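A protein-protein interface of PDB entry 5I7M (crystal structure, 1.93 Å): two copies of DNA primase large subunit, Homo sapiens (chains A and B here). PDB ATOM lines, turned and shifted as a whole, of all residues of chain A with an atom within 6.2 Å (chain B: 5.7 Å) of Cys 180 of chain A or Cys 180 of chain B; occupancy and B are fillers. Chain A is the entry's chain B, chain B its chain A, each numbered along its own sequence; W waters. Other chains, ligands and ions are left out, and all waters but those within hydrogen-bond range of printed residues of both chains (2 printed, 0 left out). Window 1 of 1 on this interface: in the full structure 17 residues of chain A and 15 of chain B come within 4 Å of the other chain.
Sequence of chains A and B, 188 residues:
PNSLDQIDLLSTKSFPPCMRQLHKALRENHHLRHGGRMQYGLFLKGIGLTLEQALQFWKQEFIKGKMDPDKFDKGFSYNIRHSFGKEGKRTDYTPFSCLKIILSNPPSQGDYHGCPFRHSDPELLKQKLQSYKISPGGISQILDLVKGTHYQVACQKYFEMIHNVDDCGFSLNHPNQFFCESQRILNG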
ATOM      1  N   SER A  14      35.464 -10.963  21.835  1.00  0.00           N
ATOM      2  CA  SER A  14      34.408  -9.956  21.984  1.00  0.00           C
ATOM      3  C   SER A  14      34.791  -8.510  22.329  1.00  0.00           C
ATOM      4  O   SER A  14      33.928  -7.632  22.306  1.00  0.00           O
ATOM      5  CB  SER A  14      33.357 -10.451  22.985  1.00  0.00           C
ATOM      6  OG  SER A  14      32.953 -11.775  22.686  1.00  0.00           O
ATOM      7  N   PRO A 175      31.821   0.999  23.377  1.00  0.00           N
ATOM      8  CA  PRO A 175      32.572  -0.280  23.455  1.00  0.00           C
ATOM      9  C   PRO A 175      31.824  -1.424  24.179  1.00  0.00           C
ATOM     10  O   PRO A 175      32.011  -2.573  23.852  1.00  0.00           O
ATOM     11  CB  PRO A 175      33.807   0.100  24.266  1.00  0.00           C
ATOM     12  CG  PRO A 175      34.029   1.568  23.929  1.00  0.00           C
ATOM     13  CD  PRO A 175      32.615   2.119  23.880  1.00  0.00           C
ATOM     14  N   ASN A 176      31.084  -1.117  25.215  1.00  0.00           N
ATOM     15  CA  ASN A 176      30.278  -2.122  25.917  1.00  0.00           C
ATOM     16  C   ASN A 176      29.130  -2.668  25.101  1.00  0.00           C
ATOM     17  O   ASN A 176      28.715  -3.786  25.336  1.00  0.00           O
ATOM     18  CB  ASN A 176      29.843  -1.616  27.299  1.00  0.00           C
ATOM     19  CG  ASN A 176      30.996  -1.560  28.290  1.00  0.00           C
ATOM     20  OD1 ASN A 176      31.729  -0.540  28.386  1.00  0.00           O
ATOM     21  ND2 ASN A 176      31.215  -2.703  28.998  1.00  0.00           N
ATOM     22  N   GLN A 177      28.683  -1.912  24.119  1.00  0.00           N
ATOM     23  CA  GLN A 177      27.667  -2.332  23.193  1.00  0.00           C
ATOM     24  C   GLN A 177      28.300  -3.356  22.239  1.00  0.00           C
ATOM     25  O   GLN A 177      27.709  -4.332  21.925  1.00  0.00           O
ATOM     26  CB  GLN A 177      27.065  -1.148  22.462  1.00  0.00           C
ATOM     27  CG  GLN A 177      26.014  -1.455  21.409  1.00  0.00           C
ATOM     28  CD  GLN A 177      25.818  -0.330  20.421  1.00  0.00           C
ATOM     29  OE1 GLN A 177      26.573   0.598  20.382  1.00  0.00           O
ATOM     30  NE2 GLN A 177      24.807  -0.433  19.633  1.00  0.00           N
ATOM     31  N   PHE A 178      29.530  -3.098  21.808  1.00  0.00           N
ATOM     32  CA  PHE A 178      30.237  -4.008  20.953  1.00  0.00           C
ATOM     33  C   PHE A 178      30.322  -5.337  21.698  1.00  0.00           C
ATOM     34  O   PHE A 178      30.051  -6.339  21.159  1.00  0.00           O
ATOM     35  CB  PHE A 178      31.643  -3.467  20.651  1.00  0.00           C
ATOM     36  CG  PHE A 178      32.486  -4.307  19.700  1.00  0.00           C
ATOM     37  CD1 PHE A 178      32.934  -5.554  20.011  1.00  0.00           C
ATOM     38  CD2 PHE A 178      32.883  -3.777  18.501  1.00  0.00           C
ATOM     39  CE1 PHE A 178      33.711  -6.262  19.123  1.00  0.00           C
ATOM     40  CE2 PHE A 178      33.656  -4.461  17.620  1.00  0.00           C
ATOM     41  CZ  PHE A 178      34.075  -5.717  17.924  1.00  0.00           C
ATOM     42  N   PHE A 179      30.716  -5.299  22.950  1.00  0.00           N
ATOM     43  CA  PHE A 179      30.855  -6.535  23.731  1.00  0.00           C
ATOM     44  C   PHE A 179      29.518  -7.272  23.866  1.00  0.00           C
ATOM     45  O   PHE A 179      29.422  -8.439  23.607  1.00  0.00           O
ATOM     46  CB  PHE A 179      31.464  -6.285  25.127  1.00  0.00           C
ATOM     47  CG  PHE A 179      31.610  -7.518  25.972  1.00  0.00           C
ATOM     48  CD1 PHE A 179      32.707  -8.308  25.839  1.00  0.00           C
ATOM     49  CD2 PHE A 179      30.647  -7.874  26.894  1.00  0.00           C
ATOM     50  CE1 PHE A 179      32.845  -9.427  26.588  1.00  0.00           C
ATOM     51  CE2 PHE A 179      30.794  -9.006  27.658  1.00  0.00           C
ATOM     52  CZ  PHE A 179      31.876  -9.774  27.491  1.00  0.00           C
ATOM     53  N   CYS A 180      28.517  -6.523  24.259  1.00  0.00           N
ATOM     54  CA  CYS A 180      27.157  -7.065  24.492  1.00  0.00           C
ATOM     55  C   CYS A 180      26.659  -7.788  23.224  1.00  0.00           C
ATOM     56  O   CYS A 180      26.173  -8.936  23.276  1.00  0.00           O
ATOM     57  CB  CYS A 180      26.197  -5.972  24.804  1.00  0.00           C
ATOM     58  SG  CYS A 180      24.593  -6.629  25.387  1.00  0.00           S
ATOM     59  N   GLU A 181      26.855  -7.124  22.080  1.00  0.00           N
ATOM     60  CA  GLU A 181      26.454  -7.694  20.746  1.00  0.00           C
ATOM     61  C   GLU A 181      27.280  -8.866  20.344  1.00  0.00           C
ATOM     62  O   GLU A 181      26.764  -9.793  19.691  1.00  0.00           O
ATOM     63  CB  GLU A 181      26.400  -6.647  19.658  1.00  0.00           C
ATOM     64  CG  GLU A 181      25.363  -5.555  19.811  1.00  0.00           C
ATOM     65  CD  GLU A 181      23.904  -6.011  19.543  1.00  0.00           C
ATOM     66  OE1 GLU A 181      23.642  -7.194  19.158  1.00  0.00           O
ATOM     67  OE2 GLU A 181      23.044  -5.154  19.707  1.00  0.00           O
ATOM     68  N   SER A 182      28.574  -8.874  20.703  1.00  0.00           N
ATOM     69  CA  SER A 182      29.424 -10.022  20.437  1.00  0.00           C
ATOM     70  C   SER A 182      28.996 -11.249  21.227  1.00  0.00           C
ATOM     71  O   SER A 182      28.886 -12.357  20.704  1.00  0.00           O
ATOM     72  CB  SER A 182      30.899  -9.688  20.700  1.00  0.00           C
ATOM     73  OG  SER A 182      31.662 -10.848  20.552  1.00  0.00           O
ATOM     74  N   GLN A 183      28.702 -11.038  22.489  1.00  0.00           N
ATOM     75  CA  GLN A 183      28.197 -12.123  23.346  1.00  0.00           C
ATOM     76  C   GLN A 183      26.904 -12.793  22.795  1.00  0.00           C
ATOM     77  O   GLN A 183      26.796 -13.986  22.894  1.00  0.00           O
ATOM     78  CB  GLN A 183      28.028 -11.636  24.783  1.00  0.00           C
ATOM     79  CG  GLN A 183      29.324 -11.390  25.489  1.00  0.00           C
ATOM     80  CD  GLN A 183      30.133 -12.661  25.609  1.00  0.00           C
ATOM     81  OE1 GLN A 183      31.100 -12.942  24.871  1.00  0.00           O
ATOM     82  NE2 GLN A 183      29.731 -13.415  26.485  1.00  0.00           N
ATOM     83  N   ARG A 184      26.037 -12.037  22.165  1.00  0.00           N
ATOM     84  CA  ARG A 184      24.834 -12.596  21.605  1.00  0.00           C
ATOM     85  C   ARG A 184      25.198 -13.566  20.497  1.00  0.00           C
ATOM     86  O   ARG A 184      24.667 -14.632  20.401  1.00  0.00           O
ATOM     87  CB  ARG A 184      23.941 -11.511  21.045  1.00  0.00           C
ATOM     88  CG  ARG A 184      23.299 -10.593  22.041  1.00  0.00           C
ATOM     89  CD  ARG A 184      22.440  -9.580  21.334  1.00  0.00           C
ATOM     90  NE  ARG A 184      21.405 -10.182  20.534  1.00  0.00           N
ATOM     91  CZ  ARG A 184      20.700  -9.537  19.623  1.00  0.00           C
ATOM     92  NH1 ARG A 184      20.912  -8.262  19.384  1.00  0.00           N
ATOM     93  NH2 ARG A 184      19.769 -10.167  18.966  1.00  0.00           N
ATOM     94  N   ILE A 185      26.134 -13.168  19.669  1.00  0.00           N
ATOM     95  CA  ILE A 185      26.547 -14.001  18.570  1.00  0.00           C
ATOM     96  C   ILE A 185      27.245 -15.256  19.032  1.00  0.00           C
ATOM     97  O   ILE A 185      26.922 -16.318  18.622  1.00  0.00           O
ATOM     98  CB  ILE A 185      27.403 -13.254  17.529  1.00  0.00           C
ATOM     99  CG1 ILE A 185      26.623 -12.120  16.890  1.00  0.00           C
ATOM    100  CG2 ILE A 185      27.884 -14.216  16.455  1.00  0.00           C
ATOM    101  CD1 ILE A 185      27.333 -11.429  15.763  1.00  0.00           C
ATOM    102  N   GLY B  46      22.857 -15.604  26.646  1.00  0.00           N
ATOM    103  CA  GLY B  46      23.110 -14.597  25.608  1.00  0.00           C
ATOM    104  C   GLY B  46      23.902 -13.387  26.085  1.00  0.00           C
ATOM    105  O   GLY B  46      24.665 -12.797  25.305  1.00  0.00           O
ATOM    106  N   PRO B 175      14.695 -10.327  22.892  1.00  0.00           N
ATOM    107  CA  PRO B 175      14.946  -9.859  24.258  1.00  0.00           C
ATOM    108  C   PRO B 175      16.460  -9.482  24.498  1.00  0.00           C
ATOM    109  O   PRO B 175      16.746  -8.518  25.216  1.00  0.00           O
ATOM    110  CB  PRO B 175      14.546 -11.090  25.090  1.00  0.00           C
ATOM    111  CG  PRO B 175      13.584 -11.856  24.252  1.00  0.00           C
ATOM    112  CD  PRO B 175      14.069 -11.651  22.867  1.00  0.00           C
ATOM    113  N   ASN B 176      17.370 -10.245  23.916  1.00  0.00           N
ATOM    114  CA  ASN B 176      18.802  -9.938  24.057  1.00  0.00           C
ATOM    115  C   ASN B 176      19.227  -8.580  23.435  1.00  0.00           C
ATOM    116  O   ASN B 176      20.138  -7.941  23.889  1.00  0.00           O
ATOM    117  CB  ASN B 176      19.674 -11.111  23.644  1.00  0.00           C
ATOM    118  CG  ASN B 176      19.589 -12.252  24.636  1.00  0.00           C
ATOM    119  OD1 ASN B 176      18.858 -13.164  24.440  1.00  0.00           O
ATOM    120  ND2 ASN B 176      20.340 -12.167  25.696  1.00  0.00           N
ATOM    121  N   GLN B 177      18.515  -8.164  22.399  1.00  0.00           N
ATOM    122  CA  GLN B 177      18.744  -6.875  21.749  1.00  0.00           C
ATOM    123  C   GLN B 177      18.253  -5.729  22.682  1.00  0.00           C
ATOM    124  O   GLN B 177      18.863  -4.733  22.859  1.00  0.00           O
ATOM    125  CB  GLN B 177      18.016  -6.883  20.414  1.00  0.00           C
ATOM    126  CG  GLN B 177      17.855  -5.551  19.702  1.00  0.00           C
ATOM    127  CD  GLN B 177      16.780  -5.601  18.636  1.00  0.00           C
ATOM    128  OE1 GLN B 177      15.810  -6.274  18.785  1.00  0.00           O
ATOM    129  NE2 GLN B 177      16.988  -4.905  17.557  1.00  0.00           N
ATOM    130  N   PHE B 178      17.110  -5.944  23.280  1.00  0.00           N
ATOM    131  CA  PHE B 178      16.532  -5.018  24.227  1.00  0.00           C
ATOM    132  C   PHE B 178      17.559  -4.703  25.312  1.00  0.00           C
ATOM    133  O   PHE B 178      17.837  -3.609  25.591  1.00  0.00           O
ATOM    134  CB  PHE B 178      15.287  -5.669  24.788  1.00  0.00           C
ATOM    135  CG  PHE B 178      14.540  -4.832  25.747  1.00  0.00           C
ATOM    136  CD1 PHE B 178      15.074  -4.504  26.946  1.00  0.00           C
ATOM    137  CD2 PHE B 178      13.270  -4.410  25.454  1.00  0.00           C
ATOM    138  CE1 PHE B 178      14.371  -3.751  27.842  1.00  0.00           C
ATOM    139  CE2 PHE B 178      12.571  -3.653  26.320  1.00  0.00           C
ATOM    140  CZ  PHE B 178      13.117  -3.313  27.518  1.00  0.00           C
ATOM    141  N   PHE B 179      18.111  -5.735  25.903  1.00  0.00           N
ATOM    142  CA  PHE B 179      19.153  -5.623  26.915  1.00  0.00           C
ATOM    143  C   PHE B 179      20.357  -4.804  26.439  1.00  0.00           C
ATOM    144  O   PHE B 179      20.755  -3.880  27.054  1.00  0.00           O
ATOM    145  CB  PHE B 179      19.667  -7.023  27.341  1.00  0.00           C
ATOM    146  CG  PHE B 179      20.794  -6.962  28.348  1.00  0.00           C
ATOM    147  CD1 PHE B 179      20.545  -6.721  29.669  1.00  0.00           C
ATOM    148  CD2 PHE B 179      22.102  -7.078  27.946  1.00  0.00           C
ATOM    149  CE1 PHE B 179      21.575  -6.595  30.572  1.00  0.00           C
ATOM    150  CE2 PHE B 179      23.127  -6.970  28.837  1.00  0.00           C
ATOM    151  CZ  PHE B 179      22.862  -6.722  30.151  1.00  0.00           C
ATOM    152  N   CYS B 180      20.930  -5.193  25.333  1.00  0.00           N
ATOM    153  CA  CYS B 180      22.146  -4.455  24.794  1.00  0.00           C
ATOM    154  C   CYS B 180      21.791  -2.962  24.541  1.00  0.00           C
ATOM    155  O   CYS B 180      22.559  -2.044  24.919  1.00  0.00           O
ATOM    156  CB  CYS B 180      22.767  -5.149  23.537  1.00  0.00           C
ATOM    157  SG  CYS B 180      23.449  -6.797  23.732  1.00  0.00           S
ATOM    158  N   GLU B 181      20.611  -2.707  23.938  1.00  0.00           N
ATOM    159  CA  GLU B 181      20.200  -1.356  23.643  1.00  0.00           C
ATOM    160  C   GLU B 181      19.929  -0.571  24.913  1.00  0.00           C
ATOM    161  O   GLU B 181      20.264   0.624  25.011  1.00  0.00           O
ATOM    162  CB  GLU B 181      18.942  -1.351  22.709  1.00  0.00           C
ATOM    163  CG  GLU B 181      19.186  -1.809  21.283  1.00  0.00           C
ATOM    164  CD  GLU B 181      19.930  -0.804  20.379  1.00  0.00           C
ATOM    165  OE1 GLU B 181      20.012   0.357  20.771  1.00  0.00           O
ATOM    166  OE2 GLU B 181      20.402  -1.197  19.269  1.00  0.00           O
ATOM    167  N   SER B 182      19.383  -1.236  25.936  1.00  0.00           N
ATOM    168  CA  SER B 182      19.135  -0.569  27.247  1.00  0.00           C
ATOM    169  C   SER B 182      20.462  -0.226  27.901  1.00  0.00           C
ATOM    170  O   SER B 182      20.662   0.927  28.347  1.00  0.00           O
ATOM    171  CB  SER B 182      18.331  -1.462  28.191  1.00  0.00           C
ATOM    172  OG  SER B 182      18.483  -1.063  29.532  1.00  0.00           O
ATOM    173  N   GLN B 183      21.376  -1.206  27.971  1.00  0.00           N
ATOM    174  CA  GLN B 183      22.699  -0.916  28.477  1.00  0.00           C
ATOM    175  C   GLN B 183      23.434   0.228  27.755  1.00  0.00           C
ATOM    176  O   GLN B 183      24.103   1.023  28.390  1.00  0.00           O
ATOM    177  CB  GLN B 183      23.582  -2.133  28.540  1.00  0.00           C
ATOM    178  CG  GLN B 183      23.115  -3.083  29.624  1.00  0.00           C
ATOM    179  CD  GLN B 183      23.397  -2.544  31.013  1.00  0.00           C
ATOM    180  OE1 GLN B 183      24.527  -2.407  31.377  1.00  0.00           O
ATOM    181  NE2 GLN B 183      22.363  -2.273  31.802  1.00  0.00           N
ATOM    182  N   ARG B 184      23.312   0.273  26.452  1.00  0.00           N
ATOM    183  CA  ARG B 184      23.956   1.344  25.692  1.00  0.00           C
ATOM    184  C   ARG B 184      23.442   2.697  26.066  1.00  0.00           C
ATOM    185  O   ARG B 184      24.223   3.590  26.223  1.00  0.00           O
ATOM    186  CB  ARG B 184      23.847   1.093  24.211  1.00  0.00           C
ATOM    187  CG  ARG B 184      24.425   2.195  23.326  1.00  0.00           C
ATOM    188  CD  ARG B 184      23.393   3.202  22.851  1.00  0.00           C
ATOM    189  NE  ARG B 184      22.557   2.619  21.808  1.00  0.00           N
ATOM    190  CZ  ARG B 184      22.892   2.468  20.530  1.00  0.00           C
ATOM    191  NH1 ARG B 184      22.038   1.870  19.696  1.00  0.00           N
ATOM    192  NH2 ARG B 184      24.111   2.871  20.079  1.00  0.00           N
ATOM    193  N   ILE B 185      22.135   2.854  26.302  1.00  0.00           N
ATOM    194  CA  ILE B 185      21.632   4.115  26.825  1.00  0.00           C
ATOM    195  C   ILE B 185      22.119   4.381  28.226  1.00  0.00           C
ATOM    196  O   ILE B 185      22.541   5.491  28.537  1.00  0.00           O
ATOM    197  CB  ILE B 185      20.066   4.144  26.848  1.00  0.00           C
ATOM    198  CG1 ILE B 185      19.528   4.295  25.429  1.00  0.00           C
ATOM    199  CG2 ILE B 185      19.543   5.270  27.736  1.00  0.00           C
ATOM    200  CD1 ILE B 185      18.021   4.200  25.338  1.00  0.00           C
HETATM  201  O   HOH W   1      22.776  -2.510  20.296  1.00  0.00           O
HETATM  202  O   HOH W   2      24.888 -10.075  25.257  1.00  0.00           O
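Of the 12 printed residues of chain A, 5 touch a printed residue of chain B. Of the 12 printed residues of chain B, 6 touch a printed residue of chain A. Among the printed residues, no Asp or Glu carboxylate lies within 4 Å of a Lys or Arg side-chain nitrogen of the other chain.
O of Gly 46 of chain B sits close to O of Gln 183 of chain A (3.4 Å). The side-chain sulfur (SG) of Cys 180 of chain B is in hydrogen-bond range of the backbone NH (N) of Glu 181 of chain A, at 3.8 Å. The guanidinium group (NH2) of Arg 184 of chain B sits at hydrogen-bond distance from the side-chain amide oxygen (OE1) of Gln 177 of chain A, at 3.4 Å. The side-chain sulfur (SG) of Cys 180 of chain A forms a disulfide with the side-chain sulfur (SG) of Cys 180 of chain B, at 2.0 Å.
Gln 177 of chain A touches Arg 184 of chain B, and with the chains exchanged Arg 184 of chain A touches Gln 177 of chain B. Cys 180 of chain A touches its own counterpart, Cys 180 of chain B. Arg 184 of chain A touches Asn 176 of chain B, but with the chains exchanged Asn 176 of chain A does not touch Arg 184 of chain B (6.5 Å). Arg 184 of chain A touches Cys 180 of chain B, but with the chains exchanged Cys 180 of chain A does not touch Arg 184 of chain B (7.1 Å). Positions printed for both chains: 175, 176, 177, 178, 179, 180, 181, 182, 183, 184 and 185.
Water W2 lies within hydrogen-bond range of the backbone carbonyl oxygen of Cys 180 of chain A (2.6 Å) and the backbone carbonyl oxygen of Gly 46 of chain B (2.7 Å). Water W1 lies within hydrogen-bond range of the side-chain carboxylate (OE2) of Glu 181 of chain A (2.7 Å), the side-chain carboxylate (OE2) of Glu 181 of chain B (2.9 Å) and the side-chain amide nitrogen (NE2) of Gln 177 of chain A (3.0 Å).
SG of Cys 180 of chain A touches CD2 of Phe 179 of chain B, at 3.6 Å. N of Arg 184 of chain A touches O of Gly 46 of chain B, 3.5 Å away. Arg 184 of chain A touches Asn 176 of chain B. NH1 of Arg 184 of chain A touches CB of Gln 177 of chain B (3.4 Å). Arg 184 of chain A touches Cys 180 of chain B (CD to SG, 3.8 Å).
The side-chain amide oxygen (OE1) of Gln 183 of chain A sits at hydrogen-bond distance from the side-chain hydroxyl (OG) of Ser 14 of chain A. NH1 of Arg 184 of chain B lies within salt-bridge range of OE1 of Glu 181 of chain B, at 2.7 Å. OE1 of Glu 181 of chain A is in salt-bridge range of NH1 of Arg 184 of chain A (2.9 Å).
Of chain B, only Phe 179 (3.6 Å) and Cys 180 (2.0 Å) come within 4 Å of Cys 180 of chain A. Cys 180 of chain B touches three residues of chain A. Printed residues of chain B within 4 Å of Glu 181 of chain A: Cys 180 (3.8 Å). Of the printed residues of chain B, Arg 184 of chain A touches Gly 46, Asn 176, Gln 177 and Cys 180. Ile 185 of chain A touches none of the printed residues of chain B. The nearest residue of chain B that does not touch Cys 180 of chain A is Gly 46 of chain B (4.6 Å). The nearest residue of chain A that does not touch Cys 180 of chain B is Gln 177 of chain A (5.0 Å). The nearest printed residue of chain A that does not touch Asn 176 of chain B is Cys 180 of chain A (4.9 Å).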
